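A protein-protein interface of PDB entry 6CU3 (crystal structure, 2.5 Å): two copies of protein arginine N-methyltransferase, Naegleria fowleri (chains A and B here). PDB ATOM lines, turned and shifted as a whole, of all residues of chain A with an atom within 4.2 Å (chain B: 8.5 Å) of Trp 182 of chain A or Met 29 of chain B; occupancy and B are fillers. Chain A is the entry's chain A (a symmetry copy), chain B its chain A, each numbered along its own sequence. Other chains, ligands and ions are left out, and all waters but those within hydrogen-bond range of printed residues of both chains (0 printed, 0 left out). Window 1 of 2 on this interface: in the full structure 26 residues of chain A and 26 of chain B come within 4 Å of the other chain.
Asp 180 of chain A touches none of the printed residues of chain B. Of the printed residues of chain B, Trp 182 of chain A touches Glu 28 and Met 29. Printed residues of chain B within 4 Å of Val 185 of chain A: Ile 64 (3.995 Å). Of the printed residues of chain B, Phe 190 of chain A touches Thr 62 (3.2 Å), Ile 64 (3.8 Å) and Ile 92 (3.7 Å). Of the printed residues of chain A, Met 29 of chain B touches Trp 182. Leu 30 of chain B touches none of the printed residues of chain A. Of the printed residues of chain A, Lys 31 of chain B touches Phe 181 (3.5 Å). The nearest printed residue of chain A that does not touch Met 29 of chain B is Ile 193 of chain A (4.003 Å).
Among the printed residues, merely in contact across the chains: Phe 190 of chain A with Thr 62 of chain B (3.2 Å), Phe 181 of chain A with Lys 31 of chain B (3.5 Å), Ile 193 of chain A with Thr 62 of chain B (3.6 Å), Ile 193 of chain A with Glu 28 of chain B (3.6 Å), Phe 190 of chain A with Ile 92 of chain B (3.7 Å), Trp 182 of chain A with Met 29 of chain B (3.7 Å), Ile 193 of chain A with Ile 92 of chain B (3.8 Å), Phe 190 of chain A with Ile 64 of chain B (3.8 Å), Trp 182 of chain A with Glu 28 of chain B (3.9 Å) and Val 185 of chain A with Ile 64 of chain B (3.995 Å).
The backbone carbonyl oxygen of Ile 92 of chain B lies within hydrogen-bond range of the side-chain amide nitrogen of Asn 96 of chain B (2.6 Å). The indole nitrogen of Trp 182 of chain A lies within hydrogen-bond range of the backbone carbonyl oxygen of Lys 178 of chain A (3.4 Å). The backbone carbonyl oxygen (O) of Trp 182 of chain A is in hydrogen-bond range of the backbone NH (N) of Phe 190 of chain A, 3.0 Å away.
Of the 14 printed residues of chain B, 6 touch a printed residue of chain A. Along chain B the printed residues that touch a printed residue of chain A span positions 28 to 92. Hydrophobic or aromatic side chains of chain A that line the printed part of chain B: Phe 181, Trp 182, Phe 190 and Ile 193. Among the printed residues, 10 pairs touch across the chains.
No position is printed for both chains. Of the 10 pairs that touch across the chains among the printed residues, none has its exchanged pair printed and touching as well.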
ATOM      1  N   LYS A 178      18.386  29.626  20.432  1.00  0.00           N
ATOM      2  CA  LYS A 178      19.273  28.698  21.112  1.00  0.00           C
ATOM      3  C   LYS A 178      18.585  27.722  22.045  1.00  0.00           C
ATOM      4  O   LYS A 178      19.241  26.784  22.513  1.00  0.00           O
ATOM      5  CB  LYS A 178      20.327  29.470  21.930  1.00  0.00           C
ATOM      6  CG  LYS A 178      21.668  29.678  21.226  1.00  0.00           C
ATOM      7  CD  LYS A 178      21.643  30.794  20.202  1.00  0.00           C
ATOM      8  CE  LYS A 178      23.026  30.904  19.542  1.00  0.00           C
ATOM      9  NZ  LYS A 178      23.313  32.239  18.966  1.00  0.00           N
ATOM     10  N   ILE A 179      17.307  27.915  22.352  1.00  0.00           N
ATOM     11  CA  ILE A 179      16.546  26.987  23.181  1.00  0.00           C
ATOM     12  C   ILE A 179      15.405  26.350  22.400  1.00  0.00           C
ATOM     13  O   ILE A 179      15.283  25.125  22.352  1.00  0.00           O
ATOM     14  CB  ILE A 179      16.029  27.673  24.464  1.00  0.00           C
ATOM     15  CG1 ILE A 179      17.201  27.998  25.390  1.00  0.00           C
ATOM     16  CG2 ILE A 179      15.042  26.781  25.183  1.00  0.00           C
ATOM     17  CD1 ILE A 179      16.881  29.034  26.408  1.00  0.00           C
ATOM     18  N   ASP A 180      14.540  27.169  21.792  1.00  0.00           N
ATOM     19  CA  ASP A 180      13.512  26.618  20.906  1.00  0.00           C
ATOM     20  C   ASP A 180      14.125  25.906  19.701  1.00  0.00           C
ATOM     21  O   ASP A 180      13.474  25.050  19.097  1.00  0.00           O
ATOM     22  CB  ASP A 180      12.574  27.730  20.434  1.00  0.00           C
ATOM     23  CG  ASP A 180      11.878  28.421  21.583  1.00  0.00           C
ATOM     24  OD1 ASP A 180      11.962  27.910  22.721  1.00  0.00           O
ATOM     25  OD2 ASP A 180      11.258  29.478  21.352  1.00  0.00           O
ATOM     26  N   PHE A 181      15.376  26.238  19.364  1.00  0.00           N
ATOM     27  CA  PHE A 181      16.085  25.620  18.253  1.00  0.00           C
ATOM     28  C   PHE A 181      16.006  24.100  18.318  1.00  0.00           C
ATOM     29  O   PHE A 181      15.918  23.436  17.278  1.00  0.00           O
ATOM     30  CB  PHE A 181      17.545  26.106  18.274  1.00  0.00           C
ATOM     31  CG  PHE A 181      18.509  25.209  17.566  1.00  0.00           C
ATOM     32  CD1 PHE A 181      18.702  25.326  16.192  1.00  0.00           C
ATOM     33  CD2 PHE A 181      19.206  24.222  18.268  1.00  0.00           C
ATOM     34  CE1 PHE A 181      19.590  24.491  15.528  1.00  0.00           C
ATOM     35  CE2 PHE A 181      20.080  23.368  17.614  1.00  0.00           C
ATOM     36  CZ  PHE A 181      20.287  23.510  16.244  1.00  0.00           C
ATOM     37  N   TRP A 182      16.008  23.532  19.528  1.00  0.00           N
ATOM     38  CA  TRP A 182      16.062  22.080  19.679  1.00  0.00           C
ATOM     39  C   TRP A 182      14.763  21.367  19.312  1.00  0.00           C
ATOM     40  O   TRP A 182      14.778  20.142  19.156  1.00  0.00           O
ATOM     41  CB  TRP A 182      16.463  21.733  21.108  1.00  0.00           C
ATOM     42  CG  TRP A 182      17.830  22.234  21.411  1.00  0.00           C
ATOM     43  CD1 TRP A 182      18.166  23.260  22.246  1.00  0.00           C
ATOM     44  CD2 TRP A 182      19.057  21.756  20.847  1.00  0.00           C
ATOM     45  NE1 TRP A 182      19.530  23.441  22.251  1.00  0.00           N
ATOM     46  CE2 TRP A 182      20.101  22.534  21.397  1.00  0.00           C
ATOM     47  CE3 TRP A 182      19.375  20.737  19.948  1.00  0.00           C
ATOM     48  CZ2 TRP A 182      21.439  22.326  21.071  1.00  0.00           C
ATOM     49  CZ3 TRP A 182      20.708  20.535  19.614  1.00  0.00           C
ATOM     50  CH2 TRP A 182      21.723  21.325  20.176  1.00  0.00           C
ATOM     51  N   ASP A 183      13.654  22.085  19.141  1.00  0.00           N
ATOM     52  CA  ASP A 183      12.417  21.413  18.762  1.00  0.00           C
ATOM     53  C   ASP A 183      12.473  20.862  17.338  1.00  0.00           C
ATOM     54  O   ASP A 183      11.842  19.835  17.054  1.00  0.00           O
ATOM     55  CB  ASP A 183      11.237  22.370  18.911  1.00  0.00           C
ATOM     56  CG  ASP A 183      10.898  22.674  20.376  1.00  0.00           C
ATOM     57  OD1 ASP A 183      10.984  21.755  21.233  1.00  0.00           O
ATOM     58  OD2 ASP A 183      10.565  23.844  20.662  1.00  0.00           O
ATOM     59  N   ASN A 184      13.228  21.508  16.437  1.00  0.00           N
ATOM     60  CA  ASN A 184      13.286  21.104  15.020  1.00  0.00           C
ATOM     61  C   ASN A 184      14.731  21.254  14.526  1.00  0.00           C
ATOM     62  O   ASN A 184      15.125  22.297  13.999  1.00  0.00           O
ATOM     63  CB  ASN A 184      12.320  21.948  14.199  1.00  0.00           C
ATOM     64  CG  ASN A 184      11.997  21.339  12.848  1.00  0.00           C
ATOM     65  OD1 ASN A 184      12.854  20.745  12.183  1.00  0.00           O
ATOM     66  ND2 ASN A 184      10.752  21.515  12.413  1.00  0.00           N
ATOM     67  N   VAL A 185      15.506  20.186  14.657  1.00  0.00           N
ATOM     68  CA  VAL A 185      16.893  20.152  14.212  1.00  0.00           C
ATOM     69  C   VAL A 185      16.927  19.351  12.913  1.00  0.00           C
ATOM     70  O   VAL A 185      16.943  18.116  12.934  1.00  0.00           O
ATOM     71  CB  VAL A 185      17.805  19.559  15.282  1.00  0.00           C
ATOM     72  CG1 VAL A 185      19.244  19.547  14.812  1.00  0.00           C
ATOM     73  CG2 VAL A 185      17.670  20.355  16.582  1.00  0.00           C
ATOM     74  N   PHE A 190      14.704  17.133  18.786  1.00  0.00           N
ATOM     75  CA  PHE A 190      15.742  17.181  19.820  1.00  0.00           C
ATOM     76  C   PHE A 190      15.233  17.797  21.130  1.00  0.00           C
ATOM     77  O   PHE A 190      15.982  18.496  21.832  1.00  0.00           O
ATOM     78  CB  PHE A 190      16.976  17.925  19.302  1.00  0.00           C
ATOM     79  CG  PHE A 190      17.940  17.042  18.520  1.00  0.00           C
ATOM     80  CD1 PHE A 190      17.516  16.355  17.375  1.00  0.00           C
ATOM     81  CD2 PHE A 190      19.255  16.898  18.930  1.00  0.00           C
ATOM     82  CE1 PHE A 190      18.401  15.543  16.667  1.00  0.00           C
ATOM     83  CE2 PHE A 190      20.123  16.093  18.254  1.00  0.00           C
ATOM     84  CZ  PHE A 190      19.701  15.400  17.105  1.00  0.00           C
ATOM     85  N   SER A 191      13.950  17.563  21.453  1.00  0.00           N
ATOM     86  CA  SER A 191      13.333  18.093  22.676  1.00  0.00           C
ATOM     87  C   SER A 191      14.105  17.719  23.928  1.00  0.00           C
ATOM     88  O   SER A 191      14.275  18.553  24.829  1.00  0.00           O
ATOM     89  CB  SER A 191      11.907  17.551  22.834  1.00  0.00           C
ATOM     90  OG  SER A 191      11.037  18.163  21.923  1.00  0.00           O
ATOM     91  N   ILE A 193      17.043  17.616  24.463  1.00  0.00           N
ATOM     92  CA  ILE A 193      18.122  18.556  24.699  1.00  0.00           C
ATOM     93  C   ILE A 193      17.591  19.875  25.227  1.00  0.00           C
ATOM     94  O   ILE A 193      18.298  20.577  25.962  1.00  0.00           O
ATOM     95  CB  ILE A 193      18.932  18.711  23.410  1.00  0.00           C
ATOM     96  CG1 ILE A 193      19.561  17.358  23.072  1.00  0.00           C
ATOM     97  CG2 ILE A 193      19.963  19.827  23.537  1.00  0.00           C
ATOM     98  CD1 ILE A 193      20.574  17.447  22.024  1.00  0.00           C
ATOM     99  N   LYS A 194      16.363  20.249  24.848  1.00  0.00           N
ATOM    100  CA  LYS A 194      15.797  21.512  25.314  1.00  0.00           C
ATOM    101  C   LYS A 194      15.688  21.534  26.834  1.00  0.00           C
ATOM    102  O   LYS A 194      16.045  22.530  27.476  1.00  0.00           O
ATOM    103  CB  LYS A 194      14.425  21.742  24.680  1.00  0.00           C
ATOM    104  CG  LYS A 194      13.921  23.185  24.752  1.00  0.00           C
ATOM    105  CD  LYS A 194      12.436  23.238  24.364  1.00  0.00           C
ATOM    106  CE  LYS A 194      11.957  24.645  24.032  1.00  0.00           C
ATOM    107  NZ  LYS A 194      10.462  24.696  23.939  1.00  0.00           N
ATOM    108  N   ALA A 197      19.008  22.462  28.189  1.00  0.00           N
ATOM    109  CA  ALA A 197      19.352  23.854  27.969  1.00  0.00           C
ATOM    110  C   ALA A 197      18.666  24.744  28.997  1.00  0.00           C
ATOM    111  O   ALA A 197      19.269  25.693  29.507  1.00  0.00           O
ATOM    112  CB  ALA A 197      18.952  24.261  26.559  1.00  0.00           C
ATOM    113  N   HIS B  26      28.266  19.618  27.982  1.00  0.00           N
ATOM    114  CA  HIS B  26      28.494  20.902  27.326  1.00  0.00           C
ATOM    115  C   HIS B  26      28.574  20.777  25.789  1.00  0.00           C
ATOM    116  O   HIS B  26      27.914  21.530  25.074  1.00  0.00           O
ATOM    117  CB  HIS B  26      29.765  21.554  27.876  1.00  0.00           C
ATOM    118  N   GLU B  27      29.382  19.832  25.284  1.00  0.00           N
ATOM    119  CA  GLU B  27      29.453  19.591  23.839  1.00  0.00           C
ATOM    120  C   GLU B  27      28.102  19.175  23.259  1.00  0.00           C
ATOM    121  O   GLU B  27      27.860  19.361  22.061  1.00  0.00           O
ATOM    122  CB  GLU B  27      30.503  18.514  23.531  1.00  0.00           C
ATOM    123  N   GLU B  28      27.220  18.635  24.100  1.00  0.00           N
ATOM    124  CA  GLU B  28      25.903  18.226  23.633  1.00  0.00           C
ATOM    125  C   GLU B  28      25.079  19.386  23.079  1.00  0.00           C
ATOM    126  O   GLU B  28      24.071  19.135  22.410  1.00  0.00           O
ATOM    127  CB  GLU B  28      25.137  17.538  24.766  1.00  0.00           C
ATOM    128  CG  GLU B  28      24.681  18.467  25.869  1.00  0.00           C
ATOM    129  CD  GLU B  28      23.266  18.171  26.317  1.00  0.00           C
ATOM    130  OE1 GLU B  28      22.373  19.003  26.059  1.00  0.00           O
ATOM    131  OE2 GLU B  28      23.039  17.102  26.925  1.00  0.00           O
ATOM    132  N   MET B  29      25.493  20.639  23.286  1.00  0.00           N
ATOM    133  CA  MET B  29      24.726  21.771  22.777  1.00  0.00           C
ATOM    134  C   MET B  29      25.447  22.591  21.714  1.00  0.00           C
ATOM    135  O   MET B  29      24.944  23.657  21.345  1.00  0.00           O
ATOM    136  CB  MET B  29      24.299  22.677  23.939  1.00  0.00           C
ATOM    137  CG  MET B  29      23.021  22.181  24.600  1.00  0.00           C
ATOM    138  SD  MET B  29      22.796  22.651  26.307  1.00  0.00           S
ATOM    139  CE  MET B  29      22.988  24.428  26.270  1.00  0.00           C
ATOM    140  N   LEU B  30      26.548  22.097  21.143  1.00  0.00           N
ATOM    141  CA  LEU B  30      27.244  22.879  20.128  1.00  0.00           C
ATOM    142  C   LEU B  30      26.462  22.877  18.817  1.00  0.00           C
ATOM    143  O   LEU B  30      26.034  21.829  18.328  1.00  0.00           O
ATOM    144  CB  LEU B  30      28.672  22.366  19.893  1.00  0.00           C
ATOM    145  CG  LEU B  30      29.401  23.104  18.736  1.00  0.00           C
ATOM    146  CD1 LEU B  30      30.068  24.397  19.203  1.00  0.00           C
ATOM    147  CD2 LEU B  30      30.410  22.224  18.004  1.00  0.00           C
ATOM    148  N   LYS B  31      26.285  24.067  18.260  1.00  0.00           N
ATOM    149  CA  LYS B  31      25.646  24.296  16.973  1.00  0.00           C
ATOM    150  C   LYS B  31      26.712  24.781  15.996  1.00  0.00           C
ATOM    151  O   LYS B  31      27.276  25.864  16.185  1.00  0.00           O
ATOM    152  CB  LYS B  31      24.555  25.367  17.092  1.00  0.00           C
ATOM    153  CG  LYS B  31      23.196  24.951  17.597  1.00  0.00           C
ATOM    154  CD  LYS B  31      22.340  26.213  17.883  1.00  0.00           C
ATOM    155  CE  LYS B  31      21.915  26.933  16.583  1.00  0.00           C
ATOM    156  NZ  LYS B  31      21.086  28.182  16.749  1.00  0.00           N
ATOM    157  N   ASP B  32      26.980  24.005  14.949  1.00  0.00           N
ATOM    158  CA  ASP B  32      27.916  24.423  13.899  1.00  0.00           C
ATOM    159  C   ASP B  32      27.197  24.154  12.574  1.00  0.00           C
ATOM    160  O   ASP B  32      27.322  23.072  11.985  1.00  0.00           O
ATOM    161  CB  ASP B  32      29.268  23.692  13.995  1.00  0.00           C
ATOM    162  CG  ASP B  32      30.337  24.295  13.077  1.00  0.00           C
ATOM    163  OD1 ASP B  32      29.984  25.088  12.171  1.00  0.00           O
ATOM    164  OD2 ASP B  32      31.532  23.968  13.257  1.00  0.00           O
ATOM    165  N   ARG B  35      29.257  23.123   9.485  1.00  0.00           N
ATOM    166  CA  ARG B  35      29.671  21.734   9.655  1.00  0.00           C
ATOM    167  C   ARG B  35      28.523  20.774   9.356  1.00  0.00           C
ATOM    168  O   ARG B  35      28.590  19.948   8.441  1.00  0.00           O
ATOM    169  CB  ARG B  35      30.186  21.522  11.082  1.00  0.00           C
ATOM    170  CG  ARG B  35      30.845  20.168  11.341  1.00  0.00           C
ATOM    171  CD  ARG B  35      29.919  19.157  12.030  1.00  0.00           C
ATOM    172  NE  ARG B  35      28.987  19.738  13.002  1.00  0.00           N
ATOM    173  CZ  ARG B  35      29.298  20.052  14.262  1.00  0.00           C
ATOM    174  NH1 ARG B  35      28.375  20.563  15.075  1.00  0.00           N
ATOM    175  NH2 ARG B  35      30.536  19.878  14.712  1.00  0.00           N
ATOM    176  N   THR B  62      25.121  13.576  20.195  1.00  0.00           N
ATOM    177  CA  THR B  62      23.682  13.391  20.388  1.00  0.00           C
ATOM    178  C   THR B  62      23.028  12.582  19.271  1.00  0.00           C
ATOM    179  O   THR B  62      21.854  12.245  19.399  1.00  0.00           O
ATOM    180  CB  THR B  62      22.966  14.736  20.525  1.00  0.00           C
ATOM    181  OG1 THR B  62      23.128  15.484  19.316  1.00  0.00           O
ATOM    182  CG2 THR B  62      23.545  15.528  21.693  1.00  0.00           C
ATOM    183  N   ILE B  64      22.876  13.199  15.607  1.00  0.00           N
ATOM    184  CA  ILE B  64      22.268  13.762  14.397  1.00  0.00           C
ATOM    185  C   ILE B  64      22.769  13.057  13.125  1.00  0.00           C
ATOM    186  O   ILE B  64      21.980  12.779  12.211  1.00  0.00           O
ATOM    187  CB  ILE B  64      22.513  15.283  14.334  1.00  0.00           C
ATOM    188  CG1 ILE B  64      21.736  15.912  13.176  1.00  0.00           C
ATOM    189  CG2 ILE B  64      24.011  15.586  14.209  1.00  0.00           C
ATOM    190  CD1 ILE B  64      20.234  15.883  13.316  1.00  0.00           C
ATOM    191  N   ILE B  85      26.810  11.186  27.091  1.00  0.00           N
ATOM    192  CA  ILE B  85      26.157  11.712  25.905  1.00  0.00           C
ATOM    193  C   ILE B  85      25.447  10.596  25.137  1.00  0.00           C
ATOM    194  O   ILE B  85      24.515  10.873  24.371  1.00  0.00           O
ATOM    195  CB  ILE B  85      27.128  12.501  25.009  1.00  0.00           C
ATOM    196  CG1 ILE B  85      26.323  13.482  24.142  1.00  0.00           C
ATOM    197  CG2 ILE B  85      27.948  11.565  24.104  1.00  0.00           C
ATOM    198  CD1 ILE B  85      27.085  14.687  23.657  1.00  0.00           C
ATOM    199  N   LYS B  88      21.821  10.395  26.241  1.00  0.00           N
ATOM    200  CA  LYS B  88      20.932  11.405  25.676  1.00  0.00           C
ATOM    201  C   LYS B  88      20.562  11.058  24.244  1.00  0.00           C
ATOM    202  O   LYS B  88      19.393  11.164  23.854  1.00  0.00           O
ATOM    203  CB  LYS B  88      21.603  12.784  25.747  1.00  0.00           C
ATOM    204  CG  LYS B  88      20.712  13.958  25.353  1.00  0.00           C
ATOM    205  CD  LYS B  88      19.310  13.850  25.964  1.00  0.00           C
ATOM    206  CE  LYS B  88      19.231  14.425  27.382  1.00  0.00           C
ATOM    207  NZ  LYS B  88      17.946  14.059  28.051  1.00  0.00           N
ATOM    208  N   ILE B  92      17.035  10.539  22.005  1.00  0.00           N
ATOM    209  CA  ILE B  92      16.747  11.282  20.779  1.00  0.00           C
ATOM    210  C   ILE B  92      16.461  10.323  19.626  1.00  0.00           C
ATOM    211  O   ILE B  92      15.617  10.595  18.761  1.00  0.00           O
ATOM    212  CB  ILE B  92      17.911  12.243  20.455  1.00  0.00           C
ATOM    213  CG1 ILE B  92      17.998  13.343  21.503  1.00  0.00           C
ATOM    214  CG2 ILE B  92      17.785  12.839  19.043  1.00  0.00           C
ATOM    215  CD1 ILE B  92      19.376  13.893  21.606  1.00  0.00           C
ATOM    216  N   ASN B  96      12.781   9.801  17.657  1.00  0.00           N
ATOM    217  CA  ASN B  96      12.757  10.014  16.227  1.00  0.00           C
ATOM    218  C   ASN B  96      12.513   8.730  15.450  1.00  0.00           C
ATOM    219  O   ASN B  96      12.599   8.742  14.219  1.00  0.00           O
ATOM    220  CB  ASN B  96      14.042  10.731  15.805  1.00  0.00           C
ATOM    221  CG  ASN B  96      14.015  12.203  16.213  1.00  0.00           C
ATOM    222  OD1 ASN B  96      13.333  13.005  15.577  1.00  0.00           O
ATOM    223  ND2 ASN B  96      14.683  12.545  17.316  1.00  0.00           N
